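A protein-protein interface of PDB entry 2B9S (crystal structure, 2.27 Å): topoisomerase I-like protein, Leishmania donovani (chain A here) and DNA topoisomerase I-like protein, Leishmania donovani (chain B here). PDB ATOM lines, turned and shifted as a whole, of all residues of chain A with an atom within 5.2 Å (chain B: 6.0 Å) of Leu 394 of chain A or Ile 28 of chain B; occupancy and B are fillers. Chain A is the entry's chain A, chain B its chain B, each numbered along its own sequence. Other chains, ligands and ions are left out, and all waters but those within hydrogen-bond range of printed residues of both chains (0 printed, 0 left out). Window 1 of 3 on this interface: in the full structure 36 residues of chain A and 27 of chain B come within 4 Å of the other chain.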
ATOM      1  N   ALA A 390       8.036 -13.055  21.797  1.00  0.00           N
ATOM      2  CA  ALA A 390       7.762 -11.653  21.508  1.00  0.00           C
ATOM      3  C   ALA A 390       8.742 -10.768  22.269  1.00  0.00           C
ATOM      4  O   ALA A 390       9.297  -9.816  21.718  1.00  0.00           O
ATOM      5  CB  ALA A 390       6.331 -11.308  21.869  1.00  0.00           C
ATOM      6  N   SER A 391       8.963 -11.120  23.533  1.00  0.00           N
ATOM      7  CA  SER A 391       9.811 -10.340  24.437  1.00  0.00           C
ATOM      8  C   SER A 391      11.301 -10.478  24.127  1.00  0.00           C
ATOM      9  O   SER A 391      12.029  -9.492  24.141  1.00  0.00           O
ATOM     10  CB  SER A 391       9.535 -10.725  25.885  1.00  0.00           C
ATOM     11  OG  SER A 391       8.354 -10.103  26.323  1.00  0.00           O
ATOM     12  N   ILE A 392      11.736 -11.697  23.840  1.00  0.00           N
ATOM     13  CA  ILE A 392      13.125 -11.964  23.505  1.00  0.00           C
ATOM     14  C   ILE A 392      13.509 -11.381  22.148  1.00  0.00           C
ATOM     15  O   ILE A 392      14.670 -11.072  21.920  1.00  0.00           O
ATOM     16  CB  ILE A 392      13.478 -13.482  23.607  1.00  0.00           C
ATOM     17  CG1 ILE A 392      14.931 -13.684  24.085  1.00  0.00           C
ATOM     18  CG2 ILE A 392      13.232 -14.213  22.273  1.00  0.00           C
ATOM     19  CD1 ILE A 392      15.328 -12.889  25.350  1.00  0.00           C
ATOM     20  N   THR A 393      12.531 -11.231  21.262  1.00  0.00           N
ATOM     21  CA  THR A 393      12.742 -10.632  19.945  1.00  0.00           C
ATOM     22  C   THR A 393      13.024  -9.124  20.057  1.00  0.00           C
ATOM     23  O   THR A 393      13.828  -8.582  19.298  1.00  0.00           O
ATOM     24  CB  THR A 393      11.525 -10.886  19.029  1.00  0.00           C
ATOM     25  OG1 THR A 393      11.471 -12.274  18.684  1.00  0.00           O
ATOM     26  CG2 THR A 393      11.588 -10.060  17.760  1.00  0.00           C
ATOM     27  N   LEU A 394      12.364  -8.452  20.997  1.00  0.00           N
ATOM     28  CA  LEU A 394      12.602  -7.023  21.205  1.00  0.00           C
ATOM     29  C   LEU A 394      13.943  -6.793  21.921  1.00  0.00           C
ATOM     30  O   LEU A 394      14.710  -5.900  21.553  1.00  0.00           O
ATOM     31  CB  LEU A 394      11.442  -6.361  21.967  1.00  0.00           C
ATOM     32  CG  LEU A 394      11.376  -4.828  21.894  1.00  0.00           C
ATOM     33  CD1 LEU A 394      10.920  -4.376  20.526  1.00  0.00           C
ATOM     34  CD2 LEU A 394      10.474  -4.222  22.961  1.00  0.00           C
ATOM     35  N   ASP A 395      14.200  -7.611  22.936  1.00  0.00           N
ATOM     36  CA  ASP A 395      15.440  -7.588  23.691  1.00  0.00           C
ATOM     37  C   ASP A 395      16.630  -7.713  22.737  1.00  0.00           C
ATOM     38  O   ASP A 395      17.456  -6.797  22.648  1.00  0.00           O
ATOM     39  CB  ASP A 395      15.431  -8.728  24.718  1.00  0.00           C
ATOM     40  CG  ASP A 395      16.388  -8.494  25.880  1.00  0.00           C
ATOM     41  OD1 ASP A 395      16.403  -7.367  26.430  1.00  0.00           O
ATOM     42  OD2 ASP A 395      17.106  -9.452  26.270  1.00  0.00           O
ATOM     43  N   ARG A 396      16.688  -8.832  22.006  1.00  0.00           N
ATOM     44  CA  ARG A 396      17.745  -9.098  21.031  1.00  0.00           C
ATOM     45  C   ARG A 396      17.960  -7.929  20.060  1.00  0.00           C
ATOM     46  O   ARG A 396      19.090  -7.509  19.849  1.00  0.00           O
ATOM     47  CB  ARG A 396      17.471 -10.394  20.276  1.00  0.00           C
ATOM     48  N   TRP A 397      16.886  -7.399  19.484  1.00  0.00           N
ATOM     49  CA  TRP A 397      16.985  -6.302  18.522  1.00  0.00           C
ATOM     50  C   TRP A 397      17.654  -5.061  19.152  1.00  0.00           C
ATOM     51  O   TRP A 397      18.546  -4.468  18.549  1.00  0.00           O
ATOM     52  CB  TRP A 397      15.593  -5.971  17.961  1.00  0.00           C
ATOM     53  CG  TRP A 397      15.501  -4.790  16.995  1.00  0.00           C
ATOM     54  CD1 TRP A 397      15.815  -3.479  17.255  1.00  0.00           C
ATOM     55  CD2 TRP A 397      15.020  -4.819  15.639  1.00  0.00           C
ATOM     56  NE1 TRP A 397      15.578  -2.702  16.145  1.00  0.00           N
ATOM     57  CE2 TRP A 397      15.091  -3.496  15.139  1.00  0.00           C
ATOM     58  CE3 TRP A 397      14.541  -5.834  14.796  1.00  0.00           C
ATOM     59  CZ2 TRP A 397      14.693  -3.159  13.836  1.00  0.00           C
ATOM     60  CZ3 TRP A 397      14.152  -5.499  13.492  1.00  0.00           C
ATOM     61  CH2 TRP A 397      14.230  -4.175  13.030  1.00  0.00           C
ATOM     62  N   PHE A 398      17.217  -4.674  20.353  1.00  0.00           N
ATOM     63  CA  PHE A 398      17.807  -3.540  21.076  1.00  0.00           C
ATOM     64  C   PHE A 398      19.301  -3.792  21.337  1.00  0.00           C
ATOM     65  O   PHE A 398      20.125  -2.885  21.208  1.00  0.00           O
ATOM     66  CB  PHE A 398      17.097  -3.283  22.419  1.00  0.00           C
ATOM     67  CG  PHE A 398      15.723  -2.657  22.302  1.00  0.00           C
ATOM     68  CD1 PHE A 398      14.836  -2.707  23.385  1.00  0.00           C
ATOM     69  CD2 PHE A 398      15.307  -2.014  21.138  1.00  0.00           C
ATOM     70  CE1 PHE A 398      13.565  -2.122  23.309  1.00  0.00           C
ATOM     71  CE2 PHE A 398      14.021  -1.430  21.055  1.00  0.00           C
ATOM     72  CZ  PHE A 398      13.160  -1.488  22.146  1.00  0.00           C
ATOM     73  N   LYS A 399      19.633  -5.036  21.680  1.00  0.00           N
ATOM     74  CA  LYS A 399      20.995  -5.422  22.060  1.00  0.00           C
ATOM     75  C   LYS A 399      21.985  -5.645  20.914  1.00  0.00           C
ATOM     76  O   LYS A 399      23.188  -5.410  21.091  1.00  0.00           O
ATOM     77  CB  LYS A 399      20.973  -6.646  22.973  1.00  0.00           C
ATOM     78  CG  LYS A 399      20.464  -6.311  24.339  1.00  0.00           C
ATOM     79  CD  LYS A 399      20.484  -7.486  25.254  1.00  0.00           C
ATOM     80  CE  LYS A 399      19.778  -7.082  26.529  1.00  0.00           C
ATOM     81  NZ  LYS A 399      20.159  -7.967  27.635  1.00  0.00           N
ATOM     82  N   PHE A 416      11.993   2.283  16.952  1.00  0.00           N
ATOM     83  CA  PHE A 416      11.122   1.503  17.811  1.00  0.00           C
ATOM     84  C   PHE A 416       9.987   0.838  17.013  1.00  0.00           C
ATOM     85  O   PHE A 416       9.792  -0.375  17.104  1.00  0.00           O
ATOM     86  CB  PHE A 416      10.545   2.364  18.934  1.00  0.00           C
ATOM     87  CG  PHE A 416       9.722   1.586  19.899  1.00  0.00           C
ATOM     88  CD1 PHE A 416       8.348   1.466  19.716  1.00  0.00           C
ATOM     89  CD2 PHE A 416      10.323   0.936  20.966  1.00  0.00           C
ATOM     90  CE1 PHE A 416       7.587   0.727  20.592  1.00  0.00           C
ATOM     91  CE2 PHE A 416       9.566   0.187  21.852  1.00  0.00           C
ATOM     92  CZ  PHE A 416       8.197   0.083  21.667  1.00  0.00           C
ATOM     93  N   ALA A 419      11.195  -2.226  15.275  1.00  0.00           N
ATOM     94  CA  ALA A 419      11.444  -3.352  16.190  1.00  0.00           C
ATOM     95  C   ALA A 419      10.120  -3.945  16.723  1.00  0.00           C
ATOM     96  O   ALA A 419      10.034  -5.150  16.966  1.00  0.00           O
ATOM     97  CB  ALA A 419      12.336  -2.918  17.335  1.00  0.00           C
ATOM     98  N   ASN A 420       9.118  -3.081  16.910  1.00  0.00           N
ATOM     99  CA  ASN A 420       7.754  -3.485  17.247  1.00  0.00           C
ATOM    100  C   ASN A 420       7.082  -4.267  16.108  1.00  0.00           C
ATOM    101  O   ASN A 420       6.377  -5.260  16.369  1.00  0.00           O
ATOM    102  CB  ASN A 420       6.908  -2.249  17.592  1.00  0.00           C
ATOM    103  CG  ASN A 420       5.653  -2.585  18.380  1.00  0.00           C
ATOM    104  OD1 ASN A 420       5.321  -3.757  18.607  1.00  0.00           O
ATOM    105  ND2 ASN A 420       4.944  -1.558  18.796  1.00  0.00           N
ATOM    106  N   VAL A 423       8.189  -7.876  15.901  1.00  0.00           N
ATOM    107  CA  VAL A 423       7.411  -8.600  16.915  1.00  0.00           C
ATOM    108  C   VAL A 423       5.991  -8.937  16.415  1.00  0.00           C
ATOM    109  O   VAL A 423       5.556 -10.075  16.531  1.00  0.00           O
ATOM    110  CB  VAL A 423       7.341  -7.785  18.251  1.00  0.00           C
ATOM    111  CG1 VAL A 423       6.509  -8.524  19.316  1.00  0.00           C
ATOM    112  CG2 VAL A 423       8.759  -7.480  18.771  1.00  0.00           C
ATOM    113  N   LYS B  19       2.348  -5.041  22.092  1.00  0.00           N
ATOM    114  CA  LYS B  19       2.716  -4.117  23.155  1.00  0.00           C
ATOM    115  C   LYS B  19       1.798  -4.275  24.370  1.00  0.00           C
ATOM    116  O   LYS B  19       2.264  -4.237  25.509  1.00  0.00           O
ATOM    117  CB  LYS B  19       2.736  -2.659  22.638  1.00  0.00           C
ATOM    118  N   ILE B  23       4.868  -8.208  25.024  1.00  0.00           N
ATOM    119  CA  ILE B  23       6.215  -7.721  25.343  1.00  0.00           C
ATOM    120  C   ILE B  23       6.288  -7.300  26.829  1.00  0.00           C
ATOM    121  O   ILE B  23       5.416  -6.583  27.315  1.00  0.00           O
ATOM    122  CB  ILE B  23       6.578  -6.514  24.475  1.00  0.00           C
ATOM    123  CG1 ILE B  23       6.450  -6.848  22.987  1.00  0.00           C
ATOM    124  CG2 ILE B  23       7.981  -6.018  24.815  1.00  0.00           C
ATOM    125  CD1 ILE B  23       6.308  -5.611  22.111  1.00  0.00           C
ATOM    126  N   ASP B  24       7.308  -7.771  27.550  1.00  0.00           N
ATOM    127  CA  ASP B  24       7.539  -7.316  28.910  1.00  0.00           C
ATOM    128  C   ASP B  24       7.647  -5.778  28.852  1.00  0.00           C
ATOM    129  O   ASP B  24       8.466  -5.241  28.093  1.00  0.00           O
ATOM    130  CB  ASP B  24       8.803  -8.002  29.453  1.00  0.00           C
ATOM    131  CG  ASP B  24       8.945  -7.897  30.967  1.00  0.00           C
ATOM    132  OD1 ASP B  24       8.624  -6.838  31.526  1.00  0.00           O
ATOM    133  OD2 ASP B  24       9.410  -8.878  31.597  1.00  0.00           O
ATOM    134  N   PRO B  25       6.764  -5.056  29.571  1.00  0.00           N
ATOM    135  CA  PRO B  25       6.792  -3.588  29.445  1.00  0.00           C
ATOM    136  C   PRO B  25       8.076  -2.951  30.028  1.00  0.00           C
ATOM    137  O   PRO B  25       8.412  -1.816  29.689  1.00  0.00           O
ATOM    138  CB  PRO B  25       5.544  -3.144  30.218  1.00  0.00           C
ATOM    139  CG  PRO B  25       5.239  -4.255  31.125  1.00  0.00           C
ATOM    140  CD  PRO B  25       5.708  -5.515  30.492  1.00  0.00           C
ATOM    141  N   ARG B  26       8.773  -3.702  30.887  1.00  0.00           N
ATOM    142  CA  ARG B  26      10.063  -3.316  31.450  1.00  0.00           C
ATOM    143  C   ARG B  26      11.161  -3.261  30.383  1.00  0.00           C
ATOM    144  O   ARG B  26      12.159  -2.556  30.554  1.00  0.00           O
ATOM    145  CB  ARG B  26      10.469  -4.287  32.567  1.00  0.00           C
ATOM    146  CG  ARG B  26       9.535  -4.304  33.750  1.00  0.00           C
ATOM    147  CD  ARG B  26       9.854  -5.406  34.746  1.00  0.00           C
ATOM    148  NE  ARG B  26       9.555  -6.738  34.223  1.00  0.00           N
ATOM    149  CZ  ARG B  26       9.512  -7.854  34.954  1.00  0.00           C
ATOM    150  NH1 ARG B  26       9.723  -7.805  36.255  1.00  0.00           N
ATOM    151  NH2 ARG B  26       9.237  -9.022  34.388  1.00  0.00           N
ATOM    152  N   ILE B  27      10.997  -4.017  29.297  1.00  0.00           N
ATOM    153  CA  ILE B  27      11.928  -3.935  28.161  1.00  0.00           C
ATOM    154  C   ILE B  27      11.781  -2.570  27.473  1.00  0.00           C
ATOM    155  O   ILE B  27      12.766  -1.877  27.233  1.00  0.00           O
ATOM    156  CB  ILE B  27      11.727  -5.092  27.135  1.00  0.00           C
ATOM    157  CG1 ILE B  27      11.888  -6.465  27.805  1.00  0.00           C
ATOM    158  CG2 ILE B  27      12.671  -4.935  25.929  1.00  0.00           C
ATOM    159  CD1 ILE B  27      11.571  -7.635  26.889  1.00  0.00           C
ATOM    160  N   ILE B  28      10.537  -2.185  27.186  1.00  0.00           N
ATOM    161  CA  ILE B  28      10.217  -0.891  26.599  1.00  0.00           C
ATOM    162  C   ILE B  28      10.634   0.288  27.501  1.00  0.00           C
ATOM    163  O   ILE B  28      11.311   1.217  27.047  1.00  0.00           O
ATOM    164  CB  ILE B  28       8.715  -0.826  26.225  1.00  0.00           C
ATOM    165  CG1 ILE B  28       8.455  -1.731  25.021  1.00  0.00           C
ATOM    166  CG2 ILE B  28       8.273   0.595  25.915  1.00  0.00           C
ATOM    167  CD1 ILE B  28       7.003  -2.037  24.780  1.00  0.00           C
ATOM    168  N   CYS B  29      10.236   0.236  28.770  1.00  0.00           N
ATOM    169  CA  CYS B  29      10.588   1.270  29.751  1.00  0.00           C
ATOM    170  C   CYS B  29      12.099   1.486  29.977  1.00  0.00           C
ATOM    171  O   CYS B  29      12.530   2.638  30.028  1.00  0.00           O
ATOM    172  CB  CYS B  29       9.850   1.032  31.068  1.00  0.00           C
ATOM    173  SG  CYS B  29       8.062   1.289  30.902  1.00  0.00           S
ATOM    174  N   SER B  30      12.882   0.406  30.101  1.00  0.00           N
ATOM    175  CA  SER B  30      14.366   0.488  30.157  1.00  0.00           C
ATOM    176  C   SER B  30      15.000   1.230  28.993  1.00  0.00           C
ATOM    177  O   SER B  30      15.837   2.124  29.186  1.00  0.00           O
ATOM    178  CB  SER B  30      15.008  -0.896  30.185  1.00  0.00           C
ATOM    179  OG  SER B  30      15.633  -1.148  31.422  1.00  0.00           O
ATOM    180  N   TRP B  31      14.609   0.832  27.785  1.00  0.00           N
ATOM    181  CA  TRP B  31      15.184   1.370  26.572  1.00  0.00           C
ATOM    182  C   TRP B  31      14.770   2.829  26.389  1.00  0.00           C
ATOM    183  O   TRP B  31      15.569   3.649  25.929  1.00  0.00           O
ATOM    184  CB  TRP B  31      14.806   0.485  25.373  1.00  0.00           C
ATOM    185  CG  TRP B  31      15.197   1.036  24.031  1.00  0.00           C
ATOM    186  CD1 TRP B  31      16.311   0.715  23.295  1.00  0.00           C
ATOM    187  CD2 TRP B  31      14.463   1.988  23.249  1.00  0.00           C
ATOM    188  NE1 TRP B  31      16.317   1.422  22.111  1.00  0.00           N
ATOM    189  CE2 TRP B  31      15.195   2.207  22.058  1.00  0.00           C
ATOM    190  CE3 TRP B  31      13.260   2.681  23.443  1.00  0.00           C
ATOM    191  CZ2 TRP B  31      14.764   3.081  21.068  1.00  0.00           C
ATOM    192  CZ3 TRP B  31      12.837   3.567  22.459  1.00  0.00           C
ATOM    193  CH2 TRP B  31      13.589   3.759  21.285  1.00  0.00           C
ATOM    194  N   ALA B  32      13.536   3.154  26.761  1.00  0.00           N
ATOM    195  CA  ALA B  32      13.037   4.528  26.652  1.00  0.00           C
ATOM    196  C   ALA B  32      13.734   5.514  27.609  1.00  0.00           C
ATOM    197  O   ALA B  32      13.882   6.696  27.277  1.00  0.00           O
ATOM    198  CB  ALA B  32      11.527   4.567  26.848  1.00  0.00           C
ATOM    199  N   LYS B  33      14.146   5.037  28.788  1.00  0.00           N
ATOM    200  CA  LYS B  33      14.867   5.879  29.746  1.00  0.00           C
ATOM    201  C   LYS B  33      16.357   5.979  29.403  1.00  0.00           C
ATOM    202  O   LYS B  33      16.983   7.013  29.650  1.00  0.00           O
ATOM    203  CB  LYS B  33      14.670   5.386  31.175  1.00  0.00           C
ATOM    204  N   ILE B  42       5.061   6.105  23.260  1.00  0.00           N
ATOM    205  CA  ILE B  42       5.017   4.650  23.064  1.00  0.00           C
ATOM    206  C   ILE B  42       3.782   4.036  23.762  1.00  0.00           C
ATOM    207  O   ILE B  42       3.020   3.292  23.136  1.00  0.00           O
ATOM    208  CB  ILE B  42       6.330   3.979  23.537  1.00  0.00           C
ATOM    209  CG1 ILE B  42       7.499   4.396  22.631  1.00  0.00           C
ATOM    210  CG2 ILE B  42       6.193   2.460  23.556  1.00  0.00           C
ATOM    211  CD1 ILE B  42       8.863   4.316  23.299  1.00  0.00           C
ATOM    212  N   PHE B  43       3.592   4.358  25.047  1.00  0.00           N
ATOM    213  CA  PHE B  43       2.392   3.978  25.792  1.00  0.00           C
ATOM    214  C   PHE B  43       1.477   5.172  25.959  1.00  0.00           C
ATOM    215  O   PHE B  43       1.905   6.223  26.440  1.00  0.00           O
ATOM    216  CB  PHE B  43       2.724   3.437  27.183  1.00  0.00           C
ATOM    217  CG  PHE B  43       3.522   2.151  27.189  1.00  0.00           C
ATOM    218  CD1 PHE B  43       4.344   1.850  28.264  1.00  0.00           C
ATOM    219  CD2 PHE B  43       3.426   1.224  26.144  1.00  0.00           C
ATOM    220  CE1 PHE B  43       5.062   0.661  28.297  1.00  0.00           C
ATOM    221  CE2 PHE B  43       4.152   0.033  26.168  1.00  0.00           C
ATOM    222  CZ  PHE B  43       4.968  -0.245  27.238  1.00  0.00           C
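OG of Ser 391 of chain A is in hydrogen-bond range of N of Asp 24 of chain B, 2.8 Å away.
The side-chain carboxylate (OD2) of Asp 24 of chain B is in salt-bridge range of the guanidinium group (NH2) of Arg 26 of chain B (2.8 Å).
Ile 23 of chain B touches Ser 391 of chain A (CA to OG, 3.3 Å).
Ile 27 of chain B touches Ser 391 of chain A (CD1 to O, 3.3 Å).
Leu 394 of chain A touches Ile 23 of chain B.
Leu 394 of chain A touches Ile 27 of chain B (CD2 to CG2, 3.8 Å).
Leu 394 of chain A touches Ile 28 of chain B (CD2 to CG1, 3.8 Å).
CE1 of Phe 398 of chain A touches CG2 of Ile 27 of chain B (3.9 Å).
Phe 398 of chain A touches Trp 31 of chain B.
Phe 416 of chain A touches Ile 28 of chain B.
CD2 of Phe 416 of chain A touches CZ3 of Trp 31 of chain B, at 3.9 Å.
Phe 416 of chain A touches Ile 42 of chain B (CZ to CG2, 3.6 Å).
Leu 394 of chain A touches just these residues of chain B: Ile 23, Ile 27 and Ile 28.
Asp 395 of chain A touches none of the printed residues of chain B.
Trp 397 of chain A touches none of the printed residues of chain B.
Of the printed residues of chain B, Phe 398 of chain A touches Ile 27 (3.9 Å) and Trp 31 (3.5 Å).
Printed residues of chain A within 4 Å of Ile 23 of chain B: Ser 391 and Leu 394.
Of chain A, only Leu 394 and Phe 416 come within 4 Å of Ile 28 of chain B.
Printed residues of chain A within 4 Å of Trp 31 of chain B: Phe 398 (3.5 Å) and Phe 416 (3.9 Å).
The nearest residue of chain B that does not touch Leu 394 of chain A is Asp 24 of chain B (5.6 Å).
The nearest printed residue of chain B that does not touch Ser 391 of chain A is Pro 25 of chain B (6.2 Å).
Of the 14 printed residues of chain B, 6 touch a printed residue of chain A.
Hydrophobic or aromatic side chains of chain B within 4 Å of the printed part of chain A: Ile 23, Ile 27, Ile 28, Trp 31 and Ile 42.
Printed residues of chain A that touch a printed residue of chain B: Ser 391, Leu 394, Phe 398 and Phe 416.
Among the printed residues, 11 pairs touch across the chains.
Among the printed residues, no Asp or Glu carboxylate lies within 4 Å of a Lys or Arg side-chain nitrogen of the other chain.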
